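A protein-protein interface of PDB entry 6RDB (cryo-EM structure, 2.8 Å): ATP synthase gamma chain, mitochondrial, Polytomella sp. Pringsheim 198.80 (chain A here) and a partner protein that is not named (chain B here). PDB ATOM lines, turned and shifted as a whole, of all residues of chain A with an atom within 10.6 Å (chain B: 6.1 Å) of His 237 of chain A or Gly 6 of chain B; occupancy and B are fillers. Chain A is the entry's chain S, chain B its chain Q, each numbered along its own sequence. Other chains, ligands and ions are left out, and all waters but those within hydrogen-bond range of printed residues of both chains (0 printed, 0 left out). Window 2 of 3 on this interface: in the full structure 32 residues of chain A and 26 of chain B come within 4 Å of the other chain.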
ATOM      1  N   ASP A 232      29.145 -33.165 -12.508  1.00  0.00           N
ATOM      2  CA  ASP A 232      28.079 -33.130 -13.498  1.00  0.00           C
ATOM      3  C   ASP A 232      27.026 -32.129 -13.053  1.00  0.00           C
ATOM      4  O   ASP A 232      26.439 -32.275 -11.979  1.00  0.00           O
ATOM      5  CB  ASP A 232      27.455 -34.509 -13.698  1.00  0.00           C
ATOM      6  CG  ASP A 232      28.301 -35.403 -14.564  1.00  0.00           C
ATOM      7  OD1 ASP A 232      29.020 -34.867 -15.434  1.00  0.00           O
ATOM      8  OD2 ASP A 232      28.241 -36.635 -14.386  1.00  0.00           O
ATOM      9  N   ILE A 233      26.793 -31.118 -13.878  1.00  0.00           N
ATOM     10  CA  ILE A 233      25.791 -30.106 -13.571  1.00  0.00           C
ATOM     11  C   ILE A 233      24.419 -30.696 -13.859  1.00  0.00           C
ATOM     12  O   ILE A 233      24.192 -31.272 -14.927  1.00  0.00           O
ATOM     13  CB  ILE A 233      26.025 -28.827 -14.385  1.00  0.00           C
ATOM     14  CG1 ILE A 233      27.484 -28.389 -14.281  1.00  0.00           C
ATOM     15  CG2 ILE A 233      25.101 -27.725 -13.904  1.00  0.00           C
ATOM     16  CD1 ILE A 233      27.926 -28.062 -12.880  1.00  0.00           C
ATOM     17  N   GLU A 234      23.510 -30.567 -12.904  1.00  0.00           N
ATOM     18  CA  GLU A 234      22.152 -31.077 -13.026  1.00  0.00           C
ATOM     19  C   GLU A 234      21.164 -29.922 -12.881  1.00  0.00           C
ATOM     20  O   GLU A 234      20.183 -29.995 -12.150  1.00  0.00           O
ATOM     21  CB  GLU A 234      21.921 -32.194 -12.006  1.00  0.00           C
ATOM     22  CG  GLU A 234      20.785 -33.193 -12.277  1.00  0.00           C
ATOM     23  CD  GLU A 234      19.490 -32.861 -11.563  1.00  0.00           C
ATOM     24  OE1 GLU A 234      19.543 -32.261 -10.475  1.00  0.00           O
ATOM     25  OE2 GLU A 234      18.414 -33.191 -12.091  1.00  0.00           O
ATOM     26  N   ALA A 235      21.442 -28.813 -13.552  1.00  0.00           N
ATOM     27  CA  ALA A 235      20.570 -27.654 -13.502  1.00  0.00           C
ATOM     28  C   ALA A 235      19.770 -27.543 -14.790  1.00  0.00           C
ATOM     29  O   ALA A 235      19.969 -28.296 -15.743  1.00  0.00           O
ATOM     30  CB  ALA A 235      21.379 -26.381 -13.262  1.00  0.00           C
ATOM     31  N   SER A 236      18.843 -26.587 -14.806  1.00  0.00           N
ATOM     32  CA  SER A 236      18.083 -26.303 -16.017  1.00  0.00           C
ATOM     33  C   SER A 236      18.973 -25.671 -17.075  1.00  0.00           C
ATOM     34  O   SER A 236      19.032 -26.138 -18.217  1.00  0.00           O
ATOM     35  CB  SER A 236      16.912 -25.377 -15.694  1.00  0.00           C
ATOM     36  OG  SER A 236      15.854 -26.079 -15.068  1.00  0.00           O
ATOM     37  N   HIS A 237      19.657 -24.607 -16.713  1.00  0.00           N
ATOM     38  CA  HIS A 237      20.507 -23.848 -17.604  1.00  0.00           C
ATOM     39  C   HIS A 237      21.973 -24.161 -17.320  1.00  0.00           C
ATOM     40  O   HIS A 237      22.303 -25.157 -16.674  1.00  0.00           O
ATOM     41  CB  HIS A 237      20.135 -22.377 -17.498  1.00  0.00           C
ATOM     42  CG  HIS A 237      18.764 -22.089 -18.018  1.00  0.00           C
ATOM     43  ND1 HIS A 237      17.621 -22.412 -17.318  1.00  0.00           N
ATOM     44  CD2 HIS A 237      18.348 -21.548 -19.186  1.00  0.00           C
ATOM     45  CE1 HIS A 237      16.561 -22.069 -18.027  1.00  0.00           C
ATOM     46  NE2 HIS A 237      16.974 -21.537 -19.162  1.00  0.00           N
ATOM     47  N   GLU A 238      22.864 -23.331 -17.855  1.00  0.00           N
ATOM     48  CA  GLU A 238      24.273 -23.670 -18.008  1.00  0.00           C
ATOM     49  C   GLU A 238      25.003 -23.707 -16.668  1.00  0.00           C
ATOM     50  O   GLU A 238      24.440 -23.466 -15.597  1.00  0.00           O
ATOM     51  CB  GLU A 238      24.960 -22.667 -18.930  1.00  0.00           C
ATOM     52  CG  GLU A 238      24.204 -22.347 -20.205  1.00  0.00           C
ATOM     53  CD  GLU A 238      23.643 -23.579 -20.872  1.00  0.00           C
ATOM     54  OE1 GLU A 238      22.402 -23.671 -20.979  1.00  0.00           O
ATOM     55  OE2 GLU A 238      24.439 -24.457 -21.264  1.00  0.00           O
ATOM     56  N   ARG A 239      26.293 -24.029 -16.740  1.00  0.00           N
ATOM     57  CA  ARG A 239      27.141 -23.915 -15.565  1.00  0.00           C
ATOM     58  C   ARG A 239      27.400 -22.458 -15.206  1.00  0.00           C
ATOM     59  O   ARG A 239      27.615 -22.139 -14.032  1.00  0.00           O
ATOM     60  CB  ARG A 239      28.452 -24.662 -15.796  1.00  0.00           C
ATOM     61  CG  ARG A 239      29.243 -24.906 -14.532  1.00  0.00           C
ATOM     62  CD  ARG A 239      30.459 -25.742 -14.796  1.00  0.00           C
ATOM     63  NE  ARG A 239      31.413 -25.075 -15.669  1.00  0.00           N
ATOM     64  CZ  ARG A 239      32.544 -25.633 -16.073  1.00  0.00           C
ATOM     65  NH1 ARG A 239      32.850 -26.857 -15.675  1.00  0.00           N
ATOM     66  NH2 ARG A 239      33.368 -24.975 -16.871  1.00  0.00           N
ATOM     67  N   SER A 240      27.361 -21.562 -16.193  1.00  0.00           N
ATOM     68  CA  SER A 240      27.642 -20.155 -15.939  1.00  0.00           C
ATOM     69  C   SER A 240      26.545 -19.471 -15.138  1.00  0.00           C
ATOM     70  O   SER A 240      26.832 -18.498 -14.436  1.00  0.00           O
ATOM     71  CB  SER A 240      27.854 -19.410 -17.258  1.00  0.00           C
ATOM     72  OG  SER A 240      26.654 -19.331 -18.008  1.00  0.00           O
ATOM     73  N   ASP A 241      25.302 -19.946 -15.221  1.00  0.00           N
ATOM     74  CA  ASP A 241      24.223 -19.362 -14.440  1.00  0.00           C
ATOM     75  C   ASP A 241      23.669 -20.280 -13.360  1.00  0.00           C
ATOM     76  O   ASP A 241      22.730 -19.882 -12.665  1.00  0.00           O
ATOM     77  CB  ASP A 241      23.086 -18.876 -15.357  1.00  0.00           C
ATOM     78  CG  ASP A 241      22.683 -19.894 -16.393  1.00  0.00           C
ATOM     79  OD1 ASP A 241      23.167 -21.033 -16.333  1.00  0.00           O
ATOM     80  OD2 ASP A 241      21.898 -19.540 -17.294  1.00  0.00           O
ATOM     81  N   VAL A 242      24.210 -21.487 -13.193  1.00  0.00           N
ATOM     82  CA  VAL A 242      23.958 -22.180 -11.935  1.00  0.00           C
ATOM     83  C   VAL A 242      24.953 -21.697 -10.887  1.00  0.00           C
ATOM     84  O   VAL A 242      24.610 -21.599  -9.708  1.00  0.00           O
ATOM     85  CB  VAL A 242      23.964 -23.718 -12.098  1.00  0.00           C
ATOM     86  CG1 VAL A 242      25.338 -24.277 -12.375  1.00  0.00           C
ATOM     87  CG2 VAL A 242      23.400 -24.389 -10.879  1.00  0.00           C
ATOM     88  N   LEU A 243      26.166 -21.311 -11.301  1.00  0.00           N
ATOM     89  CA  LEU A 243      27.114 -20.700 -10.380  1.00  0.00           C
ATOM     90  C   LEU A 243      26.712 -19.277 -10.041  1.00  0.00           C
ATOM     91  O   LEU A 243      27.094 -18.763  -8.988  1.00  0.00           O
ATOM     92  CB  LEU A 243      28.521 -20.718 -10.970  1.00  0.00           C
ATOM     93  CG  LEU A 243      29.487 -21.792 -10.480  1.00  0.00           C
ATOM     94  CD1 LEU A 243      29.037 -23.165 -10.904  1.00  0.00           C
ATOM     95  CD2 LEU A 243      30.866 -21.511 -11.021  1.00  0.00           C
ATOM     96  N   ARG A 244      25.961 -18.624 -10.927  1.00  0.00           N
ATOM     97  CA  ARG A 244      25.344 -17.351 -10.578  1.00  0.00           C
ATOM     98  C   ARG A 244      24.317 -17.539  -9.471  1.00  0.00           C
ATOM     99  O   ARG A 244      24.197 -16.699  -8.577  1.00  0.00           O
ATOM    100  CB  ARG A 244      24.715 -16.725 -11.825  1.00  0.00           C
ATOM    101  CG  ARG A 244      23.886 -15.481 -11.590  1.00  0.00           C
ATOM    102  CD  ARG A 244      24.727 -14.348 -11.062  1.00  0.00           C
ATOM    103  NE  ARG A 244      25.663 -13.845 -12.058  1.00  0.00           N
ATOM    104  CZ  ARG A 244      26.505 -12.840 -11.843  1.00  0.00           C
ATOM    105  NH1 ARG A 244      27.329 -12.444 -12.805  1.00  0.00           N
ATOM    106  NH2 ARG A 244      26.527 -12.239 -10.662  1.00  0.00           N
ATOM    107  N   ASP A 245      23.587 -18.655  -9.495  1.00  0.00           N
ATOM    108  CA  ASP A 245      22.672 -18.957  -8.403  1.00  0.00           C
ATOM    109  C   ASP A 245      23.399 -19.426  -7.153  1.00  0.00           C
ATOM    110  O   ASP A 245      22.887 -19.237  -6.047  1.00  0.00           O
ATOM    111  CB  ASP A 245      21.665 -20.028  -8.827  1.00  0.00           C
ATOM    112  CG  ASP A 245      20.735 -19.561  -9.928  1.00  0.00           C
ATOM    113  OD1 ASP A 245      20.608 -18.337 -10.134  1.00  0.00           O
ATOM    114  OD2 ASP A 245      20.118 -20.425 -10.584  1.00  0.00           O
ATOM    115  N   PRO B   4      17.937 -10.932 -19.092  1.00  0.00           N
ATOM    116  CA  PRO B   4      18.842 -11.973 -18.592  1.00  0.00           C
ATOM    117  C   PRO B   4      18.598 -13.306 -19.280  1.00  0.00           C
ATOM    118  O   PRO B   4      17.534 -13.560 -19.846  1.00  0.00           O
ATOM    119  CB  PRO B   4      18.507 -12.059 -17.097  1.00  0.00           C
ATOM    120  CG  PRO B   4      17.797 -10.811 -16.787  1.00  0.00           C
ATOM    121  CD  PRO B   4      17.011 -10.534 -18.012  1.00  0.00           C
ATOM    122  N   SER B   5      19.616 -14.158 -19.229  1.00  0.00           N
ATOM    123  CA  SER B   5      19.579 -15.480 -19.844  1.00  0.00           C
ATOM    124  C   SER B   5      19.810 -16.521 -18.757  1.00  0.00           C
ATOM    125  O   SER B   5      20.939 -16.694 -18.289  1.00  0.00           O
ATOM    126  CB  SER B   5      20.631 -15.599 -20.945  1.00  0.00           C
ATOM    127  OG  SER B   5      20.376 -14.693 -22.003  1.00  0.00           O
ATOM    128  N   GLY B   6      18.746 -17.209 -18.357  1.00  0.00           N
ATOM    129  CA  GLY B   6      18.858 -18.253 -17.369  1.00  0.00           C
ATOM    130  C   GLY B   6      17.522 -18.853 -16.994  1.00  0.00           C
ATOM    131  O   GLY B   6      16.616 -18.975 -17.823  1.00  0.00           O
ATOM    132  N   PRO B   7      17.371 -19.238 -15.719  1.00  0.00           N
ATOM    133  CA  PRO B   7      16.099 -19.809 -15.254  1.00  0.00           C
ATOM    134  C   PRO B   7      14.960 -18.803 -15.207  1.00  0.00           C
ATOM    135  O   PRO B   7      15.149 -17.627 -15.525  1.00  0.00           O
ATOM    136  CB  PRO B   7      16.439 -20.325 -13.851  1.00  0.00           C
ATOM    137  CG  PRO B   7      17.925 -20.457 -13.837  1.00  0.00           C
ATOM    138  CD  PRO B   7      18.434 -19.367 -14.709  1.00  0.00           C
ATOM    139  N   PHE B   8      13.770 -19.253 -14.801  1.00  0.00           N
ATOM    140  CA  PHE B   8      12.595 -18.396 -14.880  1.00  0.00           C
ATOM    141  C   PHE B   8      12.614 -17.281 -13.849  1.00  0.00           C
ATOM    142  O   PHE B   8      12.039 -16.218 -14.098  1.00  0.00           O
ATOM    143  CB  PHE B   8      11.315 -19.226 -14.746  1.00  0.00           C
ATOM    144  CG  PHE B   8      11.096 -19.826 -13.383  1.00  0.00           C
ATOM    145  CD1 PHE B   8      10.254 -19.214 -12.467  1.00  0.00           C
ATOM    146  CD2 PHE B   8      11.687 -21.031 -13.040  1.00  0.00           C
ATOM    147  CE1 PHE B   8      10.040 -19.771 -11.227  1.00  0.00           C
ATOM    148  CE2 PHE B   8      11.472 -21.595 -11.804  1.00  0.00           C
ATOM    149  CZ  PHE B   8      10.648 -20.964 -10.897  1.00  0.00           C
ATOM    150  N   ARG B  10      15.525 -15.884 -12.877  1.00  0.00           N
ATOM    151  CA  ARG B  10      16.641 -15.019 -13.234  1.00  0.00           C
ATOM    152  C   ARG B  10      16.314 -14.108 -14.409  1.00  0.00           C
ATOM    153  O   ARG B  10      16.747 -12.951 -14.421  1.00  0.00           O
ATOM    154  CB  ARG B  10      17.869 -15.871 -13.547  1.00  0.00           C
ATOM    155  CG  ARG B  10      19.156 -15.095 -13.648  1.00  0.00           C
ATOM    156  CD  ARG B  10      19.514 -14.455 -12.326  1.00  0.00           C
ATOM    157  NE  ARG B  10      20.012 -15.427 -11.359  1.00  0.00           N
ATOM    158  CZ  ARG B  10      20.655 -15.101 -10.244  1.00  0.00           C
ATOM    159  NH1 ARG B  10      20.884 -13.827  -9.961  1.00  0.00           N
ATOM    160  NH2 ARG B  10      21.077 -16.044  -9.416  1.00  0.00           N
ATOM    161  N   VAL B  11      15.555 -14.604 -15.392  1.00  0.00           N
ATOM    162  CA  VAL B  11      15.149 -13.780 -16.529  1.00  0.00           C
ATOM    163  C   VAL B  11      14.172 -12.697 -16.079  1.00  0.00           C
ATOM    164  O   VAL B  11      14.211 -11.563 -16.575  1.00  0.00           O
ATOM    165  CB  VAL B  11      14.565 -14.676 -17.643  1.00  0.00           C
ATOM    166  CG1 VAL B  11      14.056 -13.859 -18.821  1.00  0.00           C
ATOM    167  CG2 VAL B  11      15.614 -15.659 -18.126  1.00  0.00           C
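Of the 7 printed residues of chain B, 4 touch a printed residue of chain A.
Hydrophobic or aromatic side chains of chain B within 4 Å of the printed part of chain A: Pro 7.
Along chain B the printed residues that touch a printed residue of chain A span positions 5 to 10.
Of the 14 printed residues of chain A, 4 touch a printed residue of chain B.
Among the printed residues, Asp or Glu carboxylates within 4 Å of a Lys or Arg side-chain nitrogen of the other chain: Asp 245 of chain A with Arg 10 of chain B.
Among the printed residues, pairs that only touch across the chains: His 237 of chain A with Pro 7 of chain B (3.6 Å), Asp 241 of chain A with Gly 6 of chain B (3.3 Å) and Asp 245 of chain A with Pro 7 of chain B (3.9 Å).
His 237 of chain A touches two residues of chain B.
Of the printed residues of chain A, Gly 6 of chain B touches His 237 (2.9 Å) and Asp 241 (3.3 Å).
Printed residues of chain A within 4 Å of Arg 10 of chain B: Arg 244 and Asp 245.
Printed residues of chain B within 4 Å of Arg 244 of chain A: Arg 10.
Arg 239 of chain A touches none of the printed residues of chain B.
The nearest residue of chain B that does not touch His 237 of chain A is Phe 8 of chain B (5.1 Å).
N of Glu 238 of chain A is in hydrogen-bond range of OD1 of Asp 241 of chain A (2.8 Å).
A ring nitrogen (NE2) of His 237 of chain A lies within hydrogen-bond range of the backbone carbonyl oxygen of Gly 6 of chain B (2.9 Å).
The guanidinium group (NH2) of Arg 10 of chain B is in hydrogen-bond range of the backbone carbonyl oxygen (O) of Arg 244 of chain A.
NH2 of Arg 10 of chain B is in salt-bridge range of OD1 of Asp 245 of chain A (2.4 Å).
OD2 of Asp 241 of chain A sits close to O of Ser 5 of chain B, 3.2 Å away.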
